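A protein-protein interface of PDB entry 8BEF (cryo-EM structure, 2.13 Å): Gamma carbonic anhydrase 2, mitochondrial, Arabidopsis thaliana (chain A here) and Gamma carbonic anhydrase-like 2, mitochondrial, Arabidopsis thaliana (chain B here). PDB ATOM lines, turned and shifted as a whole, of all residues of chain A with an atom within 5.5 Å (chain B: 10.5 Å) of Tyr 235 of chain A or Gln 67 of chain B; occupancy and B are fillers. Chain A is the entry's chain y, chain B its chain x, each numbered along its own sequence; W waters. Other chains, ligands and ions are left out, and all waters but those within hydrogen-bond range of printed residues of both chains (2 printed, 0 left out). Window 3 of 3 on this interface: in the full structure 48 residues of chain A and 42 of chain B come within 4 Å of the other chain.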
ATOM      1  N   ALA A 230       2.980   2.558 -11.039  1.00  0.00           N
ATOM      2  CA  ALA A 230       3.940   2.651  -9.942  1.00  0.00           C
ATOM      3  C   ALA A 230       4.272   1.272  -9.374  1.00  0.00           C
ATOM      4  O   ALA A 230       5.446   0.953  -9.144  1.00  0.00           O
ATOM      5  CB  ALA A 230       3.403   3.574  -8.848  1.00  0.00           C
ATOM      6  N   LEU A 231       3.252   0.433  -9.161  1.00  0.00           N
ATOM      7  CA  LEU A 231       3.493  -0.898  -8.611  1.00  0.00           C
ATOM      8  C   LEU A 231       4.358  -1.738  -9.545  1.00  0.00           C
ATOM      9  O   LEU A 231       5.278  -2.431  -9.096  1.00  0.00           O
ATOM     10  CB  LEU A 231       2.167  -1.606  -8.329  1.00  0.00           C
ATOM     11  CG  LEU A 231       1.392  -1.138  -7.095  1.00  0.00           C
ATOM     12  CD1 LEU A 231      -0.005  -1.748  -7.054  1.00  0.00           C
ATOM     13  CD2 LEU A 231       2.162  -1.459  -5.825  1.00  0.00           C
ATOM     14  N   ARG A 232       4.078  -1.682 -10.849  1.00  0.00           N
ATOM     15  CA  ARG A 232       4.869  -2.417 -11.827  1.00  0.00           C
ATOM     16  C   ARG A 232       6.322  -1.971 -11.798  1.00  0.00           C
ATOM     17  O   ARG A 232       7.235  -2.805 -11.823  1.00  0.00           O
ATOM     18  CB  ARG A 232       4.276  -2.214 -13.223  1.00  0.00           C
ATOM     19  CG  ARG A 232       4.342  -3.418 -14.137  1.00  0.00           C
ATOM     20  CD  ARG A 232       3.454  -3.219 -15.360  1.00  0.00           C
ATOM     21  NE  ARG A 232       2.096  -3.700 -15.140  1.00  0.00           N
ATOM     22  CZ  ARG A 232       1.015  -2.933 -15.147  1.00  0.00           C
ATOM     23  NH1 ARG A 232       1.095  -1.628 -15.351  1.00  0.00           N
ATOM     24  NH2 ARG A 232      -0.176  -3.488 -14.937  1.00  0.00           N
ATOM     25  N   LYS A 233       6.555  -0.658 -11.733  1.00  0.00           N
ATOM     26  CA  LYS A 233       7.928  -0.167 -11.665  1.00  0.00           C
ATOM     27  C   LYS A 233       8.629  -0.647 -10.399  1.00  0.00           C
ATOM     28  O   LYS A 233       9.804  -1.027 -10.437  1.00  0.00           O
ATOM     29  CB  LYS A 233       7.947   1.360 -11.744  1.00  0.00           C
ATOM     30  CG  LYS A 233       9.307   1.932 -12.084  1.00  0.00           C
ATOM     31  CD  LYS A 233       9.203   3.330 -12.678  1.00  0.00           C
ATOM     32  CE  LYS A 233       8.504   4.287 -11.726  1.00  0.00           C
ATOM     33  NZ  LYS A 233       8.253   5.614 -12.355  1.00  0.00           N
ATOM     34  N   LYS A 234       7.921  -0.644  -9.266  1.00  0.00           N
ATOM     35  CA  LYS A 234       8.556  -1.022  -8.008  1.00  0.00           C
ATOM     36  C   LYS A 234       8.995  -2.486  -8.012  1.00  0.00           C
ATOM     37  O   LYS A 234      10.073  -2.816  -7.505  1.00  0.00           O
ATOM     38  CB  LYS A 234       7.610  -0.739  -6.838  1.00  0.00           C
ATOM     39  CG  LYS A 234       7.969  -1.463  -5.550  1.00  0.00           C
ATOM     40  CD  LYS A 234       6.955  -1.176  -4.453  1.00  0.00           C
ATOM     41  CE  LYS A 234       7.587  -1.278  -3.076  1.00  0.00           C
ATOM     42  NZ  LYS A 234       8.202  -2.619  -2.857  1.00  0.00           N
ATOM     43  N   TYR A 235       8.187  -3.373  -8.591  1.00  0.00           N
ATOM     44  CA  TYR A 235       8.440  -4.807  -8.541  1.00  0.00           C
ATOM     45  C   TYR A 235       9.061  -5.356  -9.820  1.00  0.00           C
ATOM     46  O   TYR A 235       9.073  -6.574 -10.011  1.00  0.00           O
ATOM     47  CB  TYR A 235       7.146  -5.560  -8.229  1.00  0.00           C
ATOM     48  CG  TYR A 235       6.689  -5.363  -6.810  1.00  0.00           C
ATOM     49  CD1 TYR A 235       7.161  -6.177  -5.791  1.00  0.00           C
ATOM     50  CD2 TYR A 235       5.808  -4.344  -6.484  1.00  0.00           C
ATOM     51  CE1 TYR A 235       6.755  -5.991  -4.488  1.00  0.00           C
ATOM     52  CE2 TYR A 235       5.393  -4.150  -5.185  1.00  0.00           C
ATOM     53  CZ  TYR A 235       5.870  -4.977  -4.189  1.00  0.00           C
ATOM     54  OH  TYR A 235       5.462  -4.787  -2.893  1.00  0.00           O
ATOM     55  N   ALA A 236       9.576  -4.491 -10.695  1.00  0.00           N
ATOM     56  CA  ALA A 236      10.165  -4.969 -11.940  1.00  0.00           C
ATOM     57  C   ALA A 236      11.505  -5.657 -11.710  1.00  0.00           C
ATOM     58  O   ALA A 236      11.880  -6.551 -12.475  1.00  0.00           O
ATOM     59  CB  ALA A 236      10.328  -3.811 -12.923  1.00  0.00           C
ATOM     60  N   ARG A 237      12.240  -5.257 -10.676  1.00  0.00           N
ATOM     61  CA  ARG A 237      13.527  -5.846 -10.336  1.00  0.00           C
ATOM     62  C   ARG A 237      13.509  -6.213  -8.855  1.00  0.00           C
ATOM     63  O   ARG A 237      12.531  -5.960  -8.147  1.00  0.00           O
ATOM     64  CB  ARG A 237      14.681  -4.885 -10.657  1.00  0.00           C
ATOM     65  CG  ARG A 237      14.839  -4.531 -12.130  1.00  0.00           C
ATOM     66  CD  ARG A 237      15.239  -5.733 -12.958  1.00  0.00           C
ATOM     67  NE  ARG A 237      15.413  -5.385 -14.361  1.00  0.00           N
ATOM     68  CZ  ARG A 237      15.537  -6.264 -15.344  1.00  0.00           C
ATOM     69  NH1 ARG A 237      15.501  -7.567 -15.117  1.00  0.00           N
ATOM     70  NH2 ARG A 237      15.699  -5.825 -16.590  1.00  0.00           N
ATOM     71  N   ARG A 250       9.463  -9.436   0.090  1.00  0.00           N
ATOM     72  CA  ARG A 250       8.577  -8.647  -0.749  1.00  0.00           C
ATOM     73  C   ARG A 250       7.712  -9.575  -1.587  1.00  0.00           C
ATOM     74  O   ARG A 250       8.221 -10.485  -2.247  1.00  0.00           O
ATOM     75  CB  ARG A 250       9.391  -7.711  -1.639  1.00  0.00           C
ATOM     76  CG  ARG A 250      10.439  -6.923  -0.869  1.00  0.00           C
ATOM     77  CD  ARG A 250      10.883  -5.691  -1.619  1.00  0.00           C
ATOM     78  NE  ARG A 250      11.977  -5.010  -0.937  1.00  0.00           N
ATOM     79  CZ  ARG A 250      11.819  -3.987  -0.110  1.00  0.00           C
ATOM     80  NH1 ARG A 250      10.619  -3.511   0.177  1.00  0.00           N
ATOM     81  NH2 ARG A 250      12.892  -3.424   0.440  1.00  0.00           N
ATOM     82  N   GLU A 251       6.405  -9.350  -1.554  1.00  0.00           N
ATOM     83  CA  GLU A 251       5.451 -10.168  -2.283  1.00  0.00           C
ATOM     84  C   GLU A 251       4.850  -9.362  -3.425  1.00  0.00           C
ATOM     85  O   GLU A 251       4.599  -8.163  -3.286  1.00  0.00           O
ATOM     86  CB  GLU A 251       4.345 -10.678  -1.354  1.00  0.00           C
ATOM     87  CG  GLU A 251       4.726 -11.800  -0.354  1.00  0.00           C
ATOM     88  CD  GLU A 251       5.443 -13.026  -0.942  1.00  0.00           C
ATOM     89  OE1 GLU A 251       6.106 -12.953  -1.998  1.00  0.00           O
ATOM     90  OE2 GLU A 251       5.340 -14.101  -0.314  1.00  0.00           O
ATOM     91  N   THR A 252       4.647 -10.022  -4.557  1.00  0.00           N
ATOM     92  CA  THR A 252       4.031  -9.365  -5.700  1.00  0.00           C
ATOM     93  C   THR A 252       2.583  -9.019  -5.366  1.00  0.00           C
ATOM     94  O   THR A 252       1.837  -9.887  -4.899  1.00  0.00           O
ATOM     95  CB  THR A 252       4.094 -10.266  -6.933  1.00  0.00           C
ATOM     96  OG1 THR A 252       5.463 -10.507  -7.281  1.00  0.00           O
ATOM     97  CG2 THR A 252       3.391  -9.612  -8.114  1.00  0.00           C
ATOM     98  N   PRO A 253       2.157  -7.773  -5.565  1.00  0.00           N
ATOM     99  CA  PRO A 253       0.773  -7.422  -5.261  1.00  0.00           C
ATOM    100  C   PRO A 253      -0.183  -8.168  -6.167  1.00  0.00           C
ATOM    101  O   PRO A 253       0.138  -8.461  -7.335  1.00  0.00           O
ATOM    102  CB  PRO A 253       0.727  -5.908  -5.514  1.00  0.00           C
ATOM    103  CG  PRO A 253       2.147  -5.461  -5.516  1.00  0.00           C
ATOM    104  CD  PRO A 253       2.939  -6.615  -6.023  1.00  0.00           C
ATOM    105  N   LEU A 256      -0.994  -7.363  -9.935  1.00  0.00           N
ATOM    106  CA  LEU A 256      -0.015  -7.652 -10.972  1.00  0.00           C
ATOM    107  C   LEU A 256       0.057  -9.131 -11.323  1.00  0.00           C
ATOM    108  O   LEU A 256       0.837  -9.508 -12.203  1.00  0.00           O
ATOM    109  CB  LEU A 256       1.372  -7.157 -10.542  1.00  0.00           C
ATOM    110  CG  LEU A 256       1.516  -5.648 -10.335  1.00  0.00           C
ATOM    111  CD1 LEU A 256       2.924  -5.299  -9.870  1.00  0.00           C
ATOM    112  CD2 LEU A 256       1.148  -4.886 -11.598  1.00  0.00           C
ATOM    113  N   ILE A 257      -0.732  -9.978 -10.667  1.00  0.00           N
ATOM    114  CA  ILE A 257      -0.691 -11.420 -10.875  1.00  0.00           C
ATOM    115  C   ILE A 257      -1.840 -11.820 -11.784  1.00  0.00           C
ATOM    116  O   ILE A 257      -3.000 -11.482 -11.521  1.00  0.00           O
ATOM    117  CB  ILE A 257      -0.757 -12.182  -9.540  1.00  0.00           C
ATOM    118  CG1 ILE A 257       0.433 -11.807  -8.652  1.00  0.00           C
ATOM    119  CG2 ILE A 257      -0.804 -13.682  -9.782  1.00  0.00           C
ATOM    120  CD1 ILE A 257       0.142 -11.886  -7.179  1.00  0.00           C
ATOM    121  N   LEU A 258      -1.522 -12.531 -12.853  1.00  0.00           N
ATOM    122  CA  LEU A 258      -2.548 -13.018 -13.756  1.00  0.00           C
ATOM    123  C   LEU A 258      -3.174 -14.304 -13.218  1.00  0.00           C
ATOM    124  O   LEU A 258      -2.549 -15.031 -12.443  1.00  0.00           O
ATOM    125  CB  LEU A 258      -1.961 -13.265 -15.140  1.00  0.00           C
ATOM    126  CG  LEU A 258      -1.576 -11.995 -15.900  1.00  0.00           C
ATOM    127  CD1 LEU A 258      -0.832 -12.326 -17.183  1.00  0.00           C
ATOM    128  CD2 LEU A 258      -2.805 -11.147 -16.187  1.00  0.00           C
ATOM    129  N   ILE B  62      -0.691   1.054 -25.163  1.00  0.00           N
ATOM    130  CA  ILE B  62       0.103   0.104 -24.392  1.00  0.00           C
ATOM    131  C   ILE B  62      -0.835  -0.599 -23.422  1.00  0.00           C
ATOM    132  O   ILE B  62      -1.362   0.022 -22.492  1.00  0.00           O
ATOM    133  CB  ILE B  62       1.254   0.794 -23.647  1.00  0.00           C
ATOM    134  CG1 ILE B  62       2.199   1.487 -24.632  1.00  0.00           C
ATOM    135  CG2 ILE B  62       2.004  -0.210 -22.777  1.00  0.00           C
ATOM    136  CD1 ILE B  62       2.879   0.550 -25.582  1.00  0.00           C
ATOM    137  N   ILE B  63      -1.033  -1.896 -23.624  1.00  0.00           N
ATOM    138  CA  ILE B  63      -1.901  -2.680 -22.753  1.00  0.00           C
ATOM    139  C   ILE B  63      -1.033  -3.599 -21.901  1.00  0.00           C
ATOM    140  O   ILE B  63      -0.533  -4.616 -22.398  1.00  0.00           O
ATOM    141  CB  ILE B  63      -2.932  -3.481 -23.565  1.00  0.00           C
ATOM    142  CG1 ILE B  63      -3.873  -2.536 -24.319  1.00  0.00           C
ATOM    143  CG2 ILE B  63      -3.715  -4.426 -22.660  1.00  0.00           C
ATOM    144  CD1 ILE B  63      -4.744  -1.694 -23.421  1.00  0.00           C
ATOM    145  N   PRO B  64      -0.802  -3.270 -20.633  1.00  0.00           N
ATOM    146  CA  PRO B  64      -0.105  -4.209 -19.750  1.00  0.00           C
ATOM    147  C   PRO B  64      -1.014  -5.364 -19.369  1.00  0.00           C
ATOM    148  O   PRO B  64      -2.241  -5.248 -19.370  1.00  0.00           O
ATOM    149  CB  PRO B  64       0.255  -3.354 -18.531  1.00  0.00           C
ATOM    150  CG  PRO B  64      -0.785  -2.286 -18.515  1.00  0.00           C
ATOM    151  CD  PRO B  64      -1.115  -2.001 -19.955  1.00  0.00           C
ATOM    152  N   LEU B  65      -0.393  -6.494 -19.039  1.00  0.00           N
ATOM    153  CA  LEU B  65      -1.118  -7.716 -18.678  1.00  0.00           C
ATOM    154  C   LEU B  65      -0.403  -8.304 -17.463  1.00  0.00           C
ATOM    155  O   LEU B  65       0.557  -9.064 -17.601  1.00  0.00           O
ATOM    156  CB  LEU B  65      -1.163  -8.692 -19.847  1.00  0.00           C
ATOM    157  CG  LEU B  65      -2.091  -8.333 -21.015  1.00  0.00           C
ATOM    158  CD1 LEU B  65      -2.092  -9.429 -22.064  1.00  0.00           C
ATOM    159  CD2 LEU B  65      -3.505  -8.056 -20.537  1.00  0.00           C
ATOM    160  N   GLY B  66      -0.879  -7.945 -16.273  1.00  0.00           N
ATOM    161  CA  GLY B  66      -0.197  -8.322 -15.051  1.00  0.00           C
ATOM    162  C   GLY B  66       1.132  -7.609 -14.923  1.00  0.00           C
ATOM    163  O   GLY B  66       1.173  -6.381 -14.809  1.00  0.00           O
ATOM    164  N   GLN B  67       2.228  -8.360 -14.944  1.00  0.00           N
ATOM    165  CA  GLN B  67       3.557  -7.772 -14.993  1.00  0.00           C
ATOM    166  C   GLN B  67       4.122  -7.698 -16.407  1.00  0.00           C
ATOM    167  O   GLN B  67       5.207  -7.143 -16.596  1.00  0.00           O
ATOM    168  CB  GLN B  67       4.519  -8.551 -14.092  1.00  0.00           C
ATOM    169  CG  GLN B  67       4.396  -8.199 -12.622  1.00  0.00           C
ATOM    170  CD  GLN B  67       5.476  -8.845 -11.782  1.00  0.00           C
ATOM    171  OE1 GLN B  67       6.341  -8.165 -11.233  1.00  0.00           O
ATOM    172  NE2 GLN B  67       5.433 -10.164 -11.684  1.00  0.00           N
ATOM    173  N   TRP B  68       3.415  -8.236 -17.397  1.00  0.00           N
ATOM    174  CA  TRP B  68       3.877  -8.204 -18.782  1.00  0.00           C
ATOM    175  C   TRP B  68       3.620  -6.816 -19.358  1.00  0.00           C
ATOM    176  O   TRP B  68       2.480  -6.472 -19.682  1.00  0.00           O
ATOM    177  CB  TRP B  68       3.166  -9.267 -19.612  1.00  0.00           C
ATOM    178  CG  TRP B  68       3.357 -10.673 -19.146  1.00  0.00           C
ATOM    179  CD1 TRP B  68       4.393 -11.170 -18.410  1.00  0.00           C
ATOM    180  CD2 TRP B  68       2.489 -11.779 -19.415  1.00  0.00           C
ATOM    181  NE1 TRP B  68       4.217 -12.515 -18.195  1.00  0.00           N
ATOM    182  CE2 TRP B  68       3.056 -12.913 -18.805  1.00  0.00           C
ATOM    183  CE3 TRP B  68       1.285 -11.918 -20.113  1.00  0.00           C
ATOM    184  CZ2 TRP B  68       2.460 -14.171 -18.867  1.00  0.00           C
ATOM    185  CZ3 TRP B  68       0.696 -13.168 -20.177  1.00  0.00           C
ATOM    186  CH2 TRP B  68       1.282 -14.276 -19.557  1.00  0.00           C
ATOM    187  N   LEU B  69       4.676  -6.021 -19.496  1.00  0.00           N
ATOM    188  CA  LEU B  69       4.563  -4.652 -19.978  1.00  0.00           C
ATOM    189  C   LEU B  69       5.267  -4.519 -21.320  1.00  0.00           C
ATOM    190  O   LEU B  69       6.477  -4.794 -21.408  1.00  0.00           O
ATOM    191  CB  LEU B  69       5.153  -3.671 -18.964  1.00  0.00           C
ATOM    192  CG  LEU B  69       5.154  -2.192 -19.357  1.00  0.00           C
ATOM    193  CD1 LEU B  69       3.745  -1.702 -19.647  1.00  0.00           C
ATOM    194  CD2 LEU B  69       5.803  -1.352 -18.268  1.00  0.00           C
ATOM    195  N   PRO B  70       4.572  -4.117 -22.382  1.00  0.00           N
ATOM    196  CA  PRO B  70       5.241  -3.940 -23.677  1.00  0.00           C
ATOM    197  C   PRO B  70       6.395  -2.949 -23.582  1.00  0.00           C
ATOM    198  O   PRO B  70       6.295  -1.910 -22.928  1.00  0.00           O
ATOM    199  CB  PRO B  70       4.119  -3.421 -24.582  1.00  0.00           C
ATOM    200  CG  PRO B  70       2.865  -3.954 -23.959  1.00  0.00           C
ATOM    201  CD  PRO B  70       3.112  -3.950 -22.479  1.00  0.00           C
ATOM    202  N   LYS B  71       7.498  -3.291 -24.237  1.00  0.00           N
ATOM    203  CA  LYS B  71       8.737  -2.527 -24.179  1.00  0.00           C
ATOM    204  C   LYS B  71       9.030  -1.950 -25.558  1.00  0.00           C
ATOM    205  O   LYS B  71       9.213  -2.701 -26.522  1.00  0.00           O
ATOM    206  CB  LYS B  71       9.895  -3.409 -23.710  1.00  0.00           C
ATOM    207  CG  LYS B  71      11.252  -2.715 -23.694  1.00  0.00           C
ATOM    208  CD  LYS B  71      12.329  -3.645 -23.164  1.00  0.00           C
ATOM    209  CE  LYS B  71      13.723  -3.129 -23.494  1.00  0.00           C
ATOM    210  NZ  LYS B  71      14.282  -3.746 -24.727  1.00  0.00           N
ATOM    211  N   ALA B  85       0.070  -5.375 -26.621  1.00  0.00           N
ATOM    212  CA  ALA B  85      -0.455  -5.974 -25.400  1.00  0.00           C
ATOM    213  C   ALA B  85       0.468  -7.079 -24.907  1.00  0.00           C
ATOM    214  O   ALA B  85       0.852  -7.962 -25.678  1.00  0.00           O
ATOM    215  CB  ALA B  85      -1.868  -6.521 -25.622  1.00  0.00           C
ATOM    216  N   GLY B  86       0.805  -7.028 -23.626  1.00  0.00           N
ATOM    217  CA  GLY B  86       1.506  -8.137 -22.998  1.00  0.00           C
ATOM    218  C   GLY B  86       2.976  -8.174 -23.353  1.00  0.00           C
ATOM    219  O   GLY B  86       3.666  -7.154 -23.317  1.00  0.00           O
ATOM    220  N   GLN B  87       3.458  -9.368 -23.699  1.00  0.00           N
ATOM    221  CA  GLN B  87       4.891  -9.634 -23.850  1.00  0.00           C
ATOM    222  C   GLN B  87       5.358  -9.250 -25.257  1.00  0.00           C
ATOM    223  O   GLN B  87       5.640 -10.090 -26.113  1.00  0.00           O
ATOM    224  CB  GLN B  87       5.186 -11.095 -23.540  1.00  0.00           C
ATOM    225  CG  GLN B  87       4.478 -11.618 -22.297  1.00  0.00           C
ATOM    226  CD  GLN B  87       4.436 -13.134 -22.239  1.00  0.00           C
ATOM    227  OE1 GLN B  87       5.441 -13.781 -21.957  1.00  0.00           O
ATOM    228  NE2 GLN B  87       3.266 -13.706 -22.503  1.00  0.00           N
ATOM    229  N   VAL B  88       5.455  -7.943 -25.478  1.00  0.00           N
ATOM    230  CA  VAL B  88       5.872  -7.387 -26.761  1.00  0.00           C
ATOM    231  C   VAL B  88       7.118  -6.542 -26.543  1.00  0.00           C
ATOM    232  O   VAL B  88       7.151  -5.695 -25.644  1.00  0.00           O
ATOM    233  CB  VAL B  88       4.753  -6.550 -27.408  1.00  0.00           C
ATOM    234  CG1 VAL B  88       5.241  -5.914 -28.704  1.00  0.00           C
ATOM    235  CG2 VAL B  88       3.517  -7.411 -27.647  1.00  0.00           C
ATOM    236  N   THR B  89       8.140  -6.774 -27.364  1.00  0.00           N
ATOM    237  CA  THR B  89       9.358  -5.974 -27.354  1.00  0.00           C
ATOM    238  C   THR B  89       9.596  -5.419 -28.751  1.00  0.00           C
ATOM    239  O   THR B  89       9.669  -6.178 -29.722  1.00  0.00           O
ATOM    240  CB  THR B  89      10.564  -6.795 -26.889  1.00  0.00           C
ATOM    241  OG1 THR B  89      10.241  -7.480 -25.674  1.00  0.00           O
ATOM    242  CG2 THR B  89      11.762  -5.885 -26.650  1.00  0.00           C
ATOM    243  N   GLY B 104       0.857 -10.138 -27.314  1.00  0.00           N
ATOM    244  CA  GLY B 104       1.650 -11.148 -26.644  1.00  0.00           C
ATOM    245  C   GLY B 104       1.050 -11.684 -25.359  1.00  0.00           C
ATOM    246  O   GLY B 104       1.687 -11.594 -24.307  1.00  0.00           O
ATOM    247  N   LYS B 108       5.809 -14.635 -26.219  1.00  0.00           N
ATOM    248  CA  LYS B 108       6.539 -13.403 -26.472  1.00  0.00           C
ATOM    249  C   LYS B 108       6.461 -13.013 -27.945  1.00  0.00           C
ATOM    250  O   LYS B 108       6.429 -13.864 -28.837  1.00  0.00           O
ATOM    251  CB  LYS B 108       8.004 -13.555 -26.060  1.00  0.00           C
ATOM    252  CG  LYS B 108       8.232 -13.681 -24.563  1.00  0.00           C
ATOM    253  CD  LYS B 108       9.635 -14.184 -24.275  1.00  0.00           C
ATOM    254  CE  LYS B 108       9.827 -14.506 -22.801  1.00  0.00           C
ATOM    255  NZ  LYS B 108       8.540 -14.802 -22.116  1.00  0.00           N
HETATM  256  O   HOH W   1       3.040 -11.254 -11.977  1.00  0.00           O
HETATM  257  O   HOH W   2       6.517  -5.583 -12.522  1.00  0.00           O
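The guanidinium group (NE) of Arg 232 of chain A lies within hydrogen-bond range of the backbone carbonyl oxygen (O) of Gly 66 of chain B (2.9 Å). O of Tyr 235 of chain A lies close to OE1 of Gln 67 of chain B (3.4 Å). The backbone carbonyl oxygen (O) of Leu 256 of chain A lies within hydrogen-bond range of the backbone NH (N) of Gln 67 of chain B, at 3.3 Å.
The side-chain amino group of Lys 234 of chain A is in hydrogen-bond range of the side-chain hydroxyl of Tyr 235 of chain A, 3.5 Å away.
Among the printed residues, merely in contact across the chains: Arg 232 of chain A with Pro 64 of chain B (3.5 Å), Leu 256 of chain A with Gly 66 of chain B (3.3 Å), Leu 258 of chain A with Leu 65 of chain B (3.6 Å), Leu 258 of chain A with Gly 66 of chain B (3.7 Å) and Leu 258 of chain A with Trp 68 of chain B (3.5 Å).
Tyr 235 of chain A touches one residue of chain B. Gln 67 of chain B touches just these residues of chain A: Tyr 235 and Leu 256. No residue of chain B comes within 4 Å of Leu 231 of chain A. No residue of chain B comes within 4 Å of Lys 234 of chain A. No residue of chain B comes within 4 Å of Ala 236 of chain A. No residue of chain B comes within 4 Å of Thr 252 of chain A. Leu 256 of chain A touches two residues of chain B. Printed residues of chain B within 4 Å of Leu 258 of chain A: Leu 65, Gly 66 and Trp 68. Of the printed residues of chain A, Gly 66 of chain B touches Arg 232, Leu 256 and Leu 258. Of the printed residues of chain B, Arg 232 of chain A touches Pro 64 and Gly 66. Of the printed residues of chain A, Leu 65 of chain B touches Leu 258. Of the printed residues of chain A, Trp 68 of chain B touches Leu 258 (3.5 Å). Lys 108 of chain B touches none of the printed residues of chain A. Pro 253 of chain A touches none of the printed residues of chain B. The nearest residue of chain B that does not touch Tyr 235 of chain A is Gly 66 of chain B (8.9 Å). The nearest printed residue of chain A that does not touch Pro 64 of chain B is Leu 258 of chain A (6.7 Å).
Along chain B the printed residues that touch a printed residue of chain A span positions 64 to 68. Of the 15 printed residues of chain A, 4 touch a printed residue of chain B. Hydrophobic or aromatic side chains of chain A within 4 Å of the printed part of chain B: Leu 256 and Leu 258. Along chain A the printed residues that touch a printed residue of chain B span positions 232 to 258.
Water W1 bridges NE2 of Gln 67 of chain B and O of Leu 256 of chain A. Water W2 lies within hydrogen-bond range of OE1 of Gln 67 of chain B (2.9 Å) and O of Arg 232 of chain A (3.0 Å).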
